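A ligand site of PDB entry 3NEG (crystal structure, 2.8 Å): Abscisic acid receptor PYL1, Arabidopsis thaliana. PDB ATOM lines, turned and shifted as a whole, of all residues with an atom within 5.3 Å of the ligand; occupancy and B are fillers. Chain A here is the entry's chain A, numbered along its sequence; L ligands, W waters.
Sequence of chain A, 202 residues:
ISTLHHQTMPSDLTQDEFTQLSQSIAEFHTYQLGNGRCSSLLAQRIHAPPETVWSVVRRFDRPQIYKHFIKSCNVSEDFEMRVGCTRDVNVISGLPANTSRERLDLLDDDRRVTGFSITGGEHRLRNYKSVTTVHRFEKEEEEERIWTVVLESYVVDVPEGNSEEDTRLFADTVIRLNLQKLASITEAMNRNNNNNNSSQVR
Residues that only touch the ligand: Val 89 (3.1 Å), Tyr 128 (3.2 Å), Ser 100 (3.3 Å), Ala 97 (3.3 Å), His 123 (3.5 Å), Ile 70 (3.5 Å), Leu 125 (3.5 Å), Val 174 (3.6 Å), Phe 170 (3.8 Å) and Ile 175 (3.9 Å).
Hydrophobic or aromatic side chains within 4 Å of the ligand: Ile 70, Val 89, Ala 97, His 123, Leu 125, Tyr 128, Phe 170, Val 174 and Ile 175.
Of the 23 residues printed, 12 come within 4 Å of the ligand.
The nearest printed residue that does not touch the ligand is Ile 118 (4.01 Å).
Water W1 lies within hydrogen-bond range of the side-chain carboxylate of Glu 102 (2.6 Å) and a nitrogen (N1) of the ligand (3.1 Å).
ND1 of His 123 is in hydrogen-bond range of N of Leu 125 (3.2 Å).
The side-chain amide nitrogen (ND2) of Asn 178 lies close to the backbone carbonyl oxygen (O) of Val 174 (3.2 Å).
OE2 of Glu 102 is in hydrogen-bond range of OG of Ser 100, 2.8 Å away.
The backbone carbonyl oxygen of Ser 100 sits at hydrogen-bond distance from the backbone NH of Val 89, 2.7 Å away.
O of Tyr 128 is in hydrogen-bond range of N of Ile 118 (3.0 Å).
OE2 of Glu 102 is in hydrogen-bond range of N1 of the ligand (2.7 Å).
N2 of the ligand sits close to NZ of Lys 67 (3.4 Å).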
ATOM      1  N   LYS A  67       4.717   8.748   7.208  1.00  0.00           N
ATOM      2  CA  LYS A  67       4.975   8.131   8.504  1.00  0.00           C
ATOM      3  C   LYS A  67       3.699   7.439   9.012  1.00  0.00           C
ATOM      4  O   LYS A  67       2.589   7.901   8.753  1.00  0.00           O
ATOM      5  CB  LYS A  67       5.462   9.168   9.506  1.00  0.00           C
ATOM      6  CG  LYS A  67       6.917   9.619   9.351  1.00  0.00           C
ATOM      7  CD  LYS A  67       7.131  11.005   9.977  1.00  0.00           C
ATOM      8  CE  LYS A  67       8.601  11.434   9.999  1.00  0.00           C
ATOM      9  NZ  LYS A  67       9.335  10.883  11.179  1.00  0.00           N
ATOM     10  N   HIS A  68       3.872   6.311   9.696  1.00  0.00           N
ATOM     11  CA  HIS A  68       2.773   5.568  10.273  1.00  0.00           C
ATOM     12  C   HIS A  68       2.462   6.039  11.690  1.00  0.00           C
ATOM     13  O   HIS A  68       3.265   6.711  12.330  1.00  0.00           O
ATOM     14  CB  HIS A  68       3.128   4.092  10.403  1.00  0.00           C
ATOM     15  CG  HIS A  68       3.181   3.350   9.118  1.00  0.00           C
ATOM     16  ND1 HIS A  68       4.356   3.138   8.418  1.00  0.00           N
ATOM     17  CD2 HIS A  68       2.210   2.731   8.405  1.00  0.00           C
ATOM     18  CE1 HIS A  68       4.105   2.440   7.325  1.00  0.00           C
ATOM     19  NE2 HIS A  68       2.811   2.186   7.294  1.00  0.00           N
ATOM     20  N   PHE A  69       1.273   5.661  12.163  1.00  0.00           N
ATOM     21  CA  PHE A  69       0.982   5.743  13.585  1.00  0.00           C
ATOM     22  C   PHE A  69       0.680   7.159  14.050  1.00  0.00           C
ATOM     23  O   PHE A  69       0.663   7.429  15.260  1.00  0.00           O
ATOM     24  CB  PHE A  69       2.172   5.182  14.349  1.00  0.00           C
ATOM     25  CG  PHE A  69       2.536   3.784  13.965  1.00  0.00           C
ATOM     26  CD1 PHE A  69       1.540   2.820  13.822  1.00  0.00           C
ATOM     27  CD2 PHE A  69       3.859   3.425  13.759  1.00  0.00           C
ATOM     28  CE1 PHE A  69       1.868   1.525  13.460  1.00  0.00           C
ATOM     29  CE2 PHE A  69       4.197   2.127  13.417  1.00  0.00           C
ATOM     30  CZ  PHE A  69       3.205   1.183  13.264  1.00  0.00           C
ATOM     31  N   ILE A  70       0.433   8.059  13.117  1.00  0.00           N
ATOM     32  CA  ILE A  70       0.091   9.406  13.487  1.00  0.00           C
ATOM     33  C   ILE A  70      -1.430   9.606  13.462  1.00  0.00           C
ATOM     34  O   ILE A  70      -2.078   9.378  12.446  1.00  0.00           O
ATOM     35  CB  ILE A  70       0.830  10.413  12.586  1.00  0.00           C
ATOM     36  CG1 ILE A  70       2.351  10.265  12.801  1.00  0.00           C
ATOM     37  CG2 ILE A  70       0.400  11.841  12.871  1.00  0.00           C
ATOM     38  CD1 ILE A  70       3.187  11.096  11.866  1.00  0.00           C
ATOM     39  N   VAL A  89       2.644  16.336  17.263  1.00  0.00           N
ATOM     40  CA  VAL A  89       2.099  15.166  16.620  1.00  0.00           C
ATOM     41  C   VAL A  89       1.552  14.248  17.656  1.00  0.00           C
ATOM     42  O   VAL A  89       2.181  14.027  18.695  1.00  0.00           O
ATOM     43  CB  VAL A  89       3.147  14.391  15.792  1.00  0.00           C
ATOM     44  CG1 VAL A  89       4.476  14.430  16.454  1.00  0.00           C
ATOM     45  CG2 VAL A  89       2.715  12.943  15.629  1.00  0.00           C
ATOM     46  N   VAL A  91       0.150  10.463  18.502  1.00  0.00           N
ATOM     47  CA  VAL A  91       0.207   9.070  18.093  1.00  0.00           C
ATOM     48  C   VAL A  91      -1.128   8.397  18.293  1.00  0.00           C
ATOM     49  O   VAL A  91      -1.878   8.720  19.211  1.00  0.00           O
ATOM     50  CB  VAL A  91       1.215   8.292  18.910  1.00  0.00           C
ATOM     51  CG1 VAL A  91       1.325   6.865  18.397  1.00  0.00           C
ATOM     52  CG2 VAL A  91       2.544   8.967  18.875  1.00  0.00           C
ATOM     53  N   LEU A  95      -0.377   2.719  21.570  1.00  0.00           N
ATOM     54  CA  LEU A  95       1.061   2.599  21.497  1.00  0.00           C
ATOM     55  C   LEU A  95       1.746   3.155  22.739  1.00  0.00           C
ATOM     56  O   LEU A  95       1.115   3.839  23.564  1.00  0.00           O
ATOM     57  CB  LEU A  95       1.604   3.284  20.239  1.00  0.00           C
ATOM     58  CG  LEU A  95       0.977   2.783  18.948  1.00  0.00           C
ATOM     59  CD1 LEU A  95       1.639   3.411  17.752  1.00  0.00           C
ATOM     60  CD2 LEU A  95       1.077   1.271  18.882  1.00  0.00           C
ATOM     61  N   PRO A  96       3.051   2.873  22.873  1.00  0.00           N
ATOM     62  CA  PRO A  96       3.893   3.299  23.990  1.00  0.00           C
ATOM     63  C   PRO A  96       4.344   4.741  23.878  1.00  0.00           C
ATOM     64  O   PRO A  96       5.231   5.140  24.611  1.00  0.00           O
ATOM     65  CB  PRO A  96       5.105   2.373  23.861  1.00  0.00           C
ATOM     66  CG  PRO A  96       5.205   2.132  22.401  1.00  0.00           C
ATOM     67  CD  PRO A  96       3.797   2.024  21.920  1.00  0.00           C
ATOM     68  N   ALA A  97       3.747   5.513  22.980  1.00  0.00           N
ATOM     69  CA  ALA A  97       4.005   6.941  22.927  1.00  0.00           C
ATOM     70  C   ALA A  97       2.731   7.693  22.557  1.00  0.00           C
ATOM     71  O   ALA A  97       2.063   7.353  21.583  1.00  0.00           O
ATOM     72  CB  ALA A  97       5.148   7.255  21.950  1.00  0.00           C
ATOM     73  N   THR A  99       2.181  11.572  22.674  1.00  0.00           N
ATOM     74  CA  THR A  99       2.435  12.791  21.898  1.00  0.00           C
ATOM     75  C   THR A  99       3.909  13.061  21.689  1.00  0.00           C
ATOM     76  O   THR A  99       4.752  12.625  22.470  1.00  0.00           O
ATOM     77  CB  THR A  99       1.876  14.043  22.570  1.00  0.00           C
ATOM     78  OG1 THR A  99       2.430  14.142  23.879  1.00  0.00           O
ATOM     79  CG2 THR A  99       0.391  13.960  22.652  1.00  0.00           C
ATOM     80  N   SER A 100       4.205  13.807  20.626  1.00  0.00           N
ATOM     81  CA  SER A 100       5.566  14.213  20.320  1.00  0.00           C
ATOM     82  C   SER A 100       5.552  15.645  19.806  1.00  0.00           C
ATOM     83  O   SER A 100       4.680  16.018  19.017  1.00  0.00           O
ATOM     84  CB  SER A 100       6.171  13.262  19.286  1.00  0.00           C
ATOM     85  OG  SER A 100       7.475  13.637  18.926  1.00  0.00           O
ATOM     86  N   GLU A 102       8.120  18.299  17.845  1.00  0.00           N
ATOM     87  CA  GLU A 102       9.331  18.204  17.070  1.00  0.00           C
ATOM     88  C   GLU A 102       9.661  19.534  16.427  1.00  0.00           C
ATOM     89  O   GLU A 102       8.764  20.259  16.013  1.00  0.00           O
ATOM     90  CB  GLU A 102       9.147  17.121  16.029  1.00  0.00           C
ATOM     91  CG  GLU A 102       8.683  15.810  16.680  1.00  0.00           C
ATOM     92  CD  GLU A 102       8.261  14.739  15.685  1.00  0.00           C
ATOM     93  OE1 GLU A 102       8.201  15.049  14.478  1.00  0.00           O
ATOM     94  OE2 GLU A 102       7.981  13.603  16.123  1.00  0.00           O
ATOM     95  N   PHE A 116      14.951  16.900  11.949  1.00  0.00           N
ATOM     96  CA  PHE A 116      14.228  17.485  13.054  1.00  0.00           C
ATOM     97  C   PHE A 116      14.733  16.934  14.385  1.00  0.00           C
ATOM     98  O   PHE A 116      15.394  15.900  14.411  1.00  0.00           O
ATOM     99  CB  PHE A 116      12.757  17.172  12.905  1.00  0.00           C
ATOM    100  CG  PHE A 116      12.441  15.712  13.055  1.00  0.00           C
ATOM    101  CD1 PHE A 116      12.090  15.190  14.289  1.00  0.00           C
ATOM    102  CD2 PHE A 116      12.462  14.865  11.967  1.00  0.00           C
ATOM    103  CE1 PHE A 116      11.797  13.852  14.428  1.00  0.00           C
ATOM    104  CE2 PHE A 116      12.154  13.531  12.100  1.00  0.00           C
ATOM    105  CZ  PHE A 116      11.834  13.029  13.334  1.00  0.00           C
ATOM    106  N   ILE A 118      13.335  16.078  18.593  1.00  0.00           N
ATOM    107  CA  ILE A 118      12.176  15.861  19.432  1.00  0.00           C
ATOM    108  C   ILE A 118      12.382  16.542  20.787  1.00  0.00           C
ATOM    109  O   ILE A 118      13.294  16.188  21.527  1.00  0.00           O
ATOM    110  CB  ILE A 118      11.935  14.365  19.610  1.00  0.00           C
ATOM    111  CG1 ILE A 118      11.664  13.740  18.252  1.00  0.00           C
ATOM    112  CG2 ILE A 118      10.774  14.132  20.551  1.00  0.00           C
ATOM    113  CD1 ILE A 118      10.665  12.589  18.254  1.00  0.00           C
ATOM    114  N   HIS A 123       6.715  10.410  25.641  1.00  0.00           N
ATOM    115  CA  HIS A 123       7.394   9.240  25.069  1.00  0.00           C
ATOM    116  C   HIS A 123       8.766   9.043  25.688  1.00  0.00           C
ATOM    117  O   HIS A 123       9.183   9.809  26.549  1.00  0.00           O
ATOM    118  CB  HIS A 123       7.561   9.423  23.563  1.00  0.00           C
ATOM    119  CG  HIS A 123       8.320  10.658  23.205  1.00  0.00           C
ATOM    120  ND1 HIS A 123       9.626  10.865  23.600  1.00  0.00           N
ATOM    121  CD2 HIS A 123       7.958  11.749  22.494  1.00  0.00           C
ATOM    122  CE1 HIS A 123      10.031  12.032  23.150  1.00  0.00           C
ATOM    123  NE2 HIS A 123       9.046  12.598  22.477  1.00  0.00           N
ATOM    124  N   LEU A 125      11.884   8.668  23.858  1.00  0.00           N
ATOM    125  CA  LEU A 125      12.987   8.900  22.933  1.00  0.00           C
ATOM    126  C   LEU A 125      13.560  10.298  23.203  1.00  0.00           C
ATOM    127  O   LEU A 125      13.432  11.193  22.369  1.00  0.00           O
ATOM    128  CB  LEU A 125      12.516   8.754  21.488  1.00  0.00           C
ATOM    129  CG  LEU A 125      12.129   7.322  21.064  1.00  0.00           C
ATOM    130  CD1 LEU A 125      11.815   7.191  19.553  1.00  0.00           C
ATOM    131  CD2 LEU A 125      13.236   6.362  21.428  1.00  0.00           C
ATOM    132  N   TYR A 128      16.070  12.913  20.723  1.00  0.00           N
ATOM    133  CA  TYR A 128      16.192  12.311  19.410  1.00  0.00           C
ATOM    134  C   TYR A 128      16.462  13.415  18.392  1.00  0.00           C
ATOM    135  O   TYR A 128      15.850  14.479  18.425  1.00  0.00           O
ATOM    136  CB  TYR A 128      14.883  11.619  19.126  1.00  0.00           C
ATOM    137  CG  TYR A 128      14.728  10.911  17.818  1.00  0.00           C
ATOM    138  CD1 TYR A 128      14.847   9.538  17.735  1.00  0.00           C
ATOM    139  CD2 TYR A 128      14.377  11.608  16.673  1.00  0.00           C
ATOM    140  CE1 TYR A 128      14.672   8.875  16.534  1.00  0.00           C
ATOM    141  CE2 TYR A 128      14.187  10.950  15.466  1.00  0.00           C
ATOM    142  CZ  TYR A 128      14.347   9.581  15.398  1.00  0.00           C
ATOM    143  OH  TYR A 128      14.176   8.938  14.187  1.00  0.00           O
ATOM    144  N   GLU A 152      18.254   7.678   6.282  1.00  0.00           N
ATOM    145  CA  GLU A 152      17.766   8.340   7.471  1.00  0.00           C
ATOM    146  C   GLU A 152      18.604   7.865   8.631  1.00  0.00           C
ATOM    147  O   GLU A 152      18.833   6.674   8.789  1.00  0.00           O
ATOM    148  CB  GLU A 152      16.287   8.061   7.733  1.00  0.00           C
ATOM    149  CG  GLU A 152      15.751   8.867   8.910  1.00  0.00           C
ATOM    150  CD  GLU A 152      14.232   8.978   8.954  1.00  0.00           C
ATOM    151  OE1 GLU A 152      13.611   9.027   7.863  1.00  0.00           O
ATOM    152  OE2 GLU A 152      13.657   9.042  10.081  1.00  0.00           O
ATOM    153  N   PHE A 170      13.837  -0.490  18.399  1.00  0.00           N
ATOM    154  CA  PHE A 170      12.643   0.345  18.451  1.00  0.00           C
ATOM    155  C   PHE A 170      12.623   1.404  17.362  1.00  0.00           C
ATOM    156  O   PHE A 170      11.869   1.305  16.413  1.00  0.00           O
ATOM    157  CB  PHE A 170      12.576   1.009  19.820  1.00  0.00           C
ATOM    158  CG  PHE A 170      11.352   1.865  20.018  1.00  0.00           C
ATOM    159  CD1 PHE A 170      10.097   1.377  19.758  1.00  0.00           C
ATOM    160  CD2 PHE A 170      11.469   3.152  20.495  1.00  0.00           C
ATOM    161  CE1 PHE A 170       8.991   2.155  19.945  1.00  0.00           C
ATOM    162  CE2 PHE A 170      10.358   3.931  20.695  1.00  0.00           C
ATOM    163  CZ  PHE A 170       9.125   3.443  20.412  1.00  0.00           C
ATOM    164  N   ALA A 171      13.477   2.416  17.505  1.00  0.00           N
ATOM    165  CA  ALA A 171      13.563   3.500  16.520  1.00  0.00           C
ATOM    166  C   ALA A 171      13.705   2.951  15.106  1.00  0.00           C
ATOM    167  O   ALA A 171      12.963   3.350  14.201  1.00  0.00           O
ATOM    168  CB  ALA A 171      14.726   4.409  16.843  1.00  0.00           C
ATOM    169  N   VAL A 174      10.285   1.942  13.484  1.00  0.00           N
ATOM    170  CA  VAL A 174       9.426   3.028  13.061  1.00  0.00           C
ATOM    171  C   VAL A 174       9.964   3.606  11.766  1.00  0.00           C
ATOM    172  O   VAL A 174       9.228   3.819  10.803  1.00  0.00           O
ATOM    173  CB  VAL A 174       9.370   4.111  14.142  1.00  0.00           C
ATOM    174  CG1 VAL A 174       8.623   5.341  13.622  1.00  0.00           C
ATOM    175  CG2 VAL A 174       8.705   3.551  15.394  1.00  0.00           C
ATOM    176  N   ILE A 175      11.275   3.826  11.733  1.00  0.00           N
ATOM    177  CA  ILE A 175      11.855   4.452  10.576  1.00  0.00           C
ATOM    178  C   ILE A 175      11.757   3.507   9.405  1.00  0.00           C
ATOM    179  O   ILE A 175      11.404   3.901   8.288  1.00  0.00           O
ATOM    180  CB  ILE A 175      13.318   4.801  10.785  1.00  0.00           C
ATOM    181  CG1 ILE A 175      13.458   5.862  11.867  1.00  0.00           C
ATOM    182  CG2 ILE A 175      13.900   5.339   9.498  1.00  0.00           C
ATOM    183  CD1 ILE A 175      14.869   6.218  12.154  1.00  0.00           C
ATOM    184  N   ASN A 178       8.280   3.496   8.045  1.00  0.00           N
ATOM    185  CA  ASN A 178       8.028   4.769   7.421  1.00  0.00           C
ATOM    186  C   ASN A 178       8.577   4.813   6.006  1.00  0.00           C
ATOM    187  O   ASN A 178       7.873   5.201   5.064  1.00  0.00           O
ATOM    188  CB  ASN A 178       8.608   5.893   8.253  1.00  0.00           C
ATOM    189  CG  ASN A 178       7.827   6.116   9.505  1.00  0.00           C
ATOM    190  OD1 ASN A 178       6.702   5.641   9.636  1.00  0.00           O
ATOM    191  ND2 ASN A 178       8.408   6.848  10.433  1.00  0.00           N
HETATM  192  S1  LIG L   1       6.278  10.571  15.627  1.00  0.00           S
HETATM  193 BR1  LIG L   1       6.221   4.851  18.332  1.00  0.00          BR
HETATM  194  C1  LIG L   1       6.248   6.557  17.526  1.00  0.00           C
HETATM  195  N1  LIG L   1       7.791  11.011  15.449  1.00  0.00           N
HETATM  196  O1  LIG L   1       5.673  11.541  16.490  1.00  0.00           O
HETATM  197  C2  LIG L   1       6.862   7.687  18.269  1.00  0.00           C
HETATM  198  N2  LIG L   1      10.219   8.883  13.778  1.00  0.00           N
HETATM  199  O2  LIG L   1       5.610  10.486  14.365  1.00  0.00           O
HETATM  200  C3  LIG L   1       6.854   9.018  17.652  1.00  0.00           C
HETATM  201  C4  LIG L   1       6.253   9.143  16.310  1.00  0.00           C
HETATM  202  C5  LIG L   1       5.680   8.043  15.676  1.00  0.00           C
HETATM  203  C6  LIG L   1       5.681   6.770  16.274  1.00  0.00           C
HETATM  204  C7  LIG L   1       7.412  10.106  18.297  1.00  0.00           C
HETATM  205  C8  LIG L   1       7.977   9.915  19.552  1.00  0.00           C
HETATM  206  C9  LIG L   1       7.981   8.668  20.162  1.00  0.00           C
HETATM  207  C10 LIG L   1       7.431   7.551  19.524  1.00  0.00           C
HETATM  208  C11 LIG L   1       8.529  10.624  14.270  1.00  0.00           C
HETATM  209  C12 LIG L   1       9.518   9.572  14.691  1.00  0.00           C
HETATM  210  C13 LIG L   1      11.084   7.943  14.140  1.00  0.00           C
HETATM  211  C14 LIG L   1      11.309   7.649  15.475  1.00  0.00           C
HETATM  212  C15 LIG L   1      10.610   8.352  16.440  1.00  0.00           C
HETATM  213  C16 LIG L   1       9.712   9.328  16.044  1.00  0.00           C
HETATM  214  O   HOH W   1       6.971  13.104  13.288  1.00  0.00           O
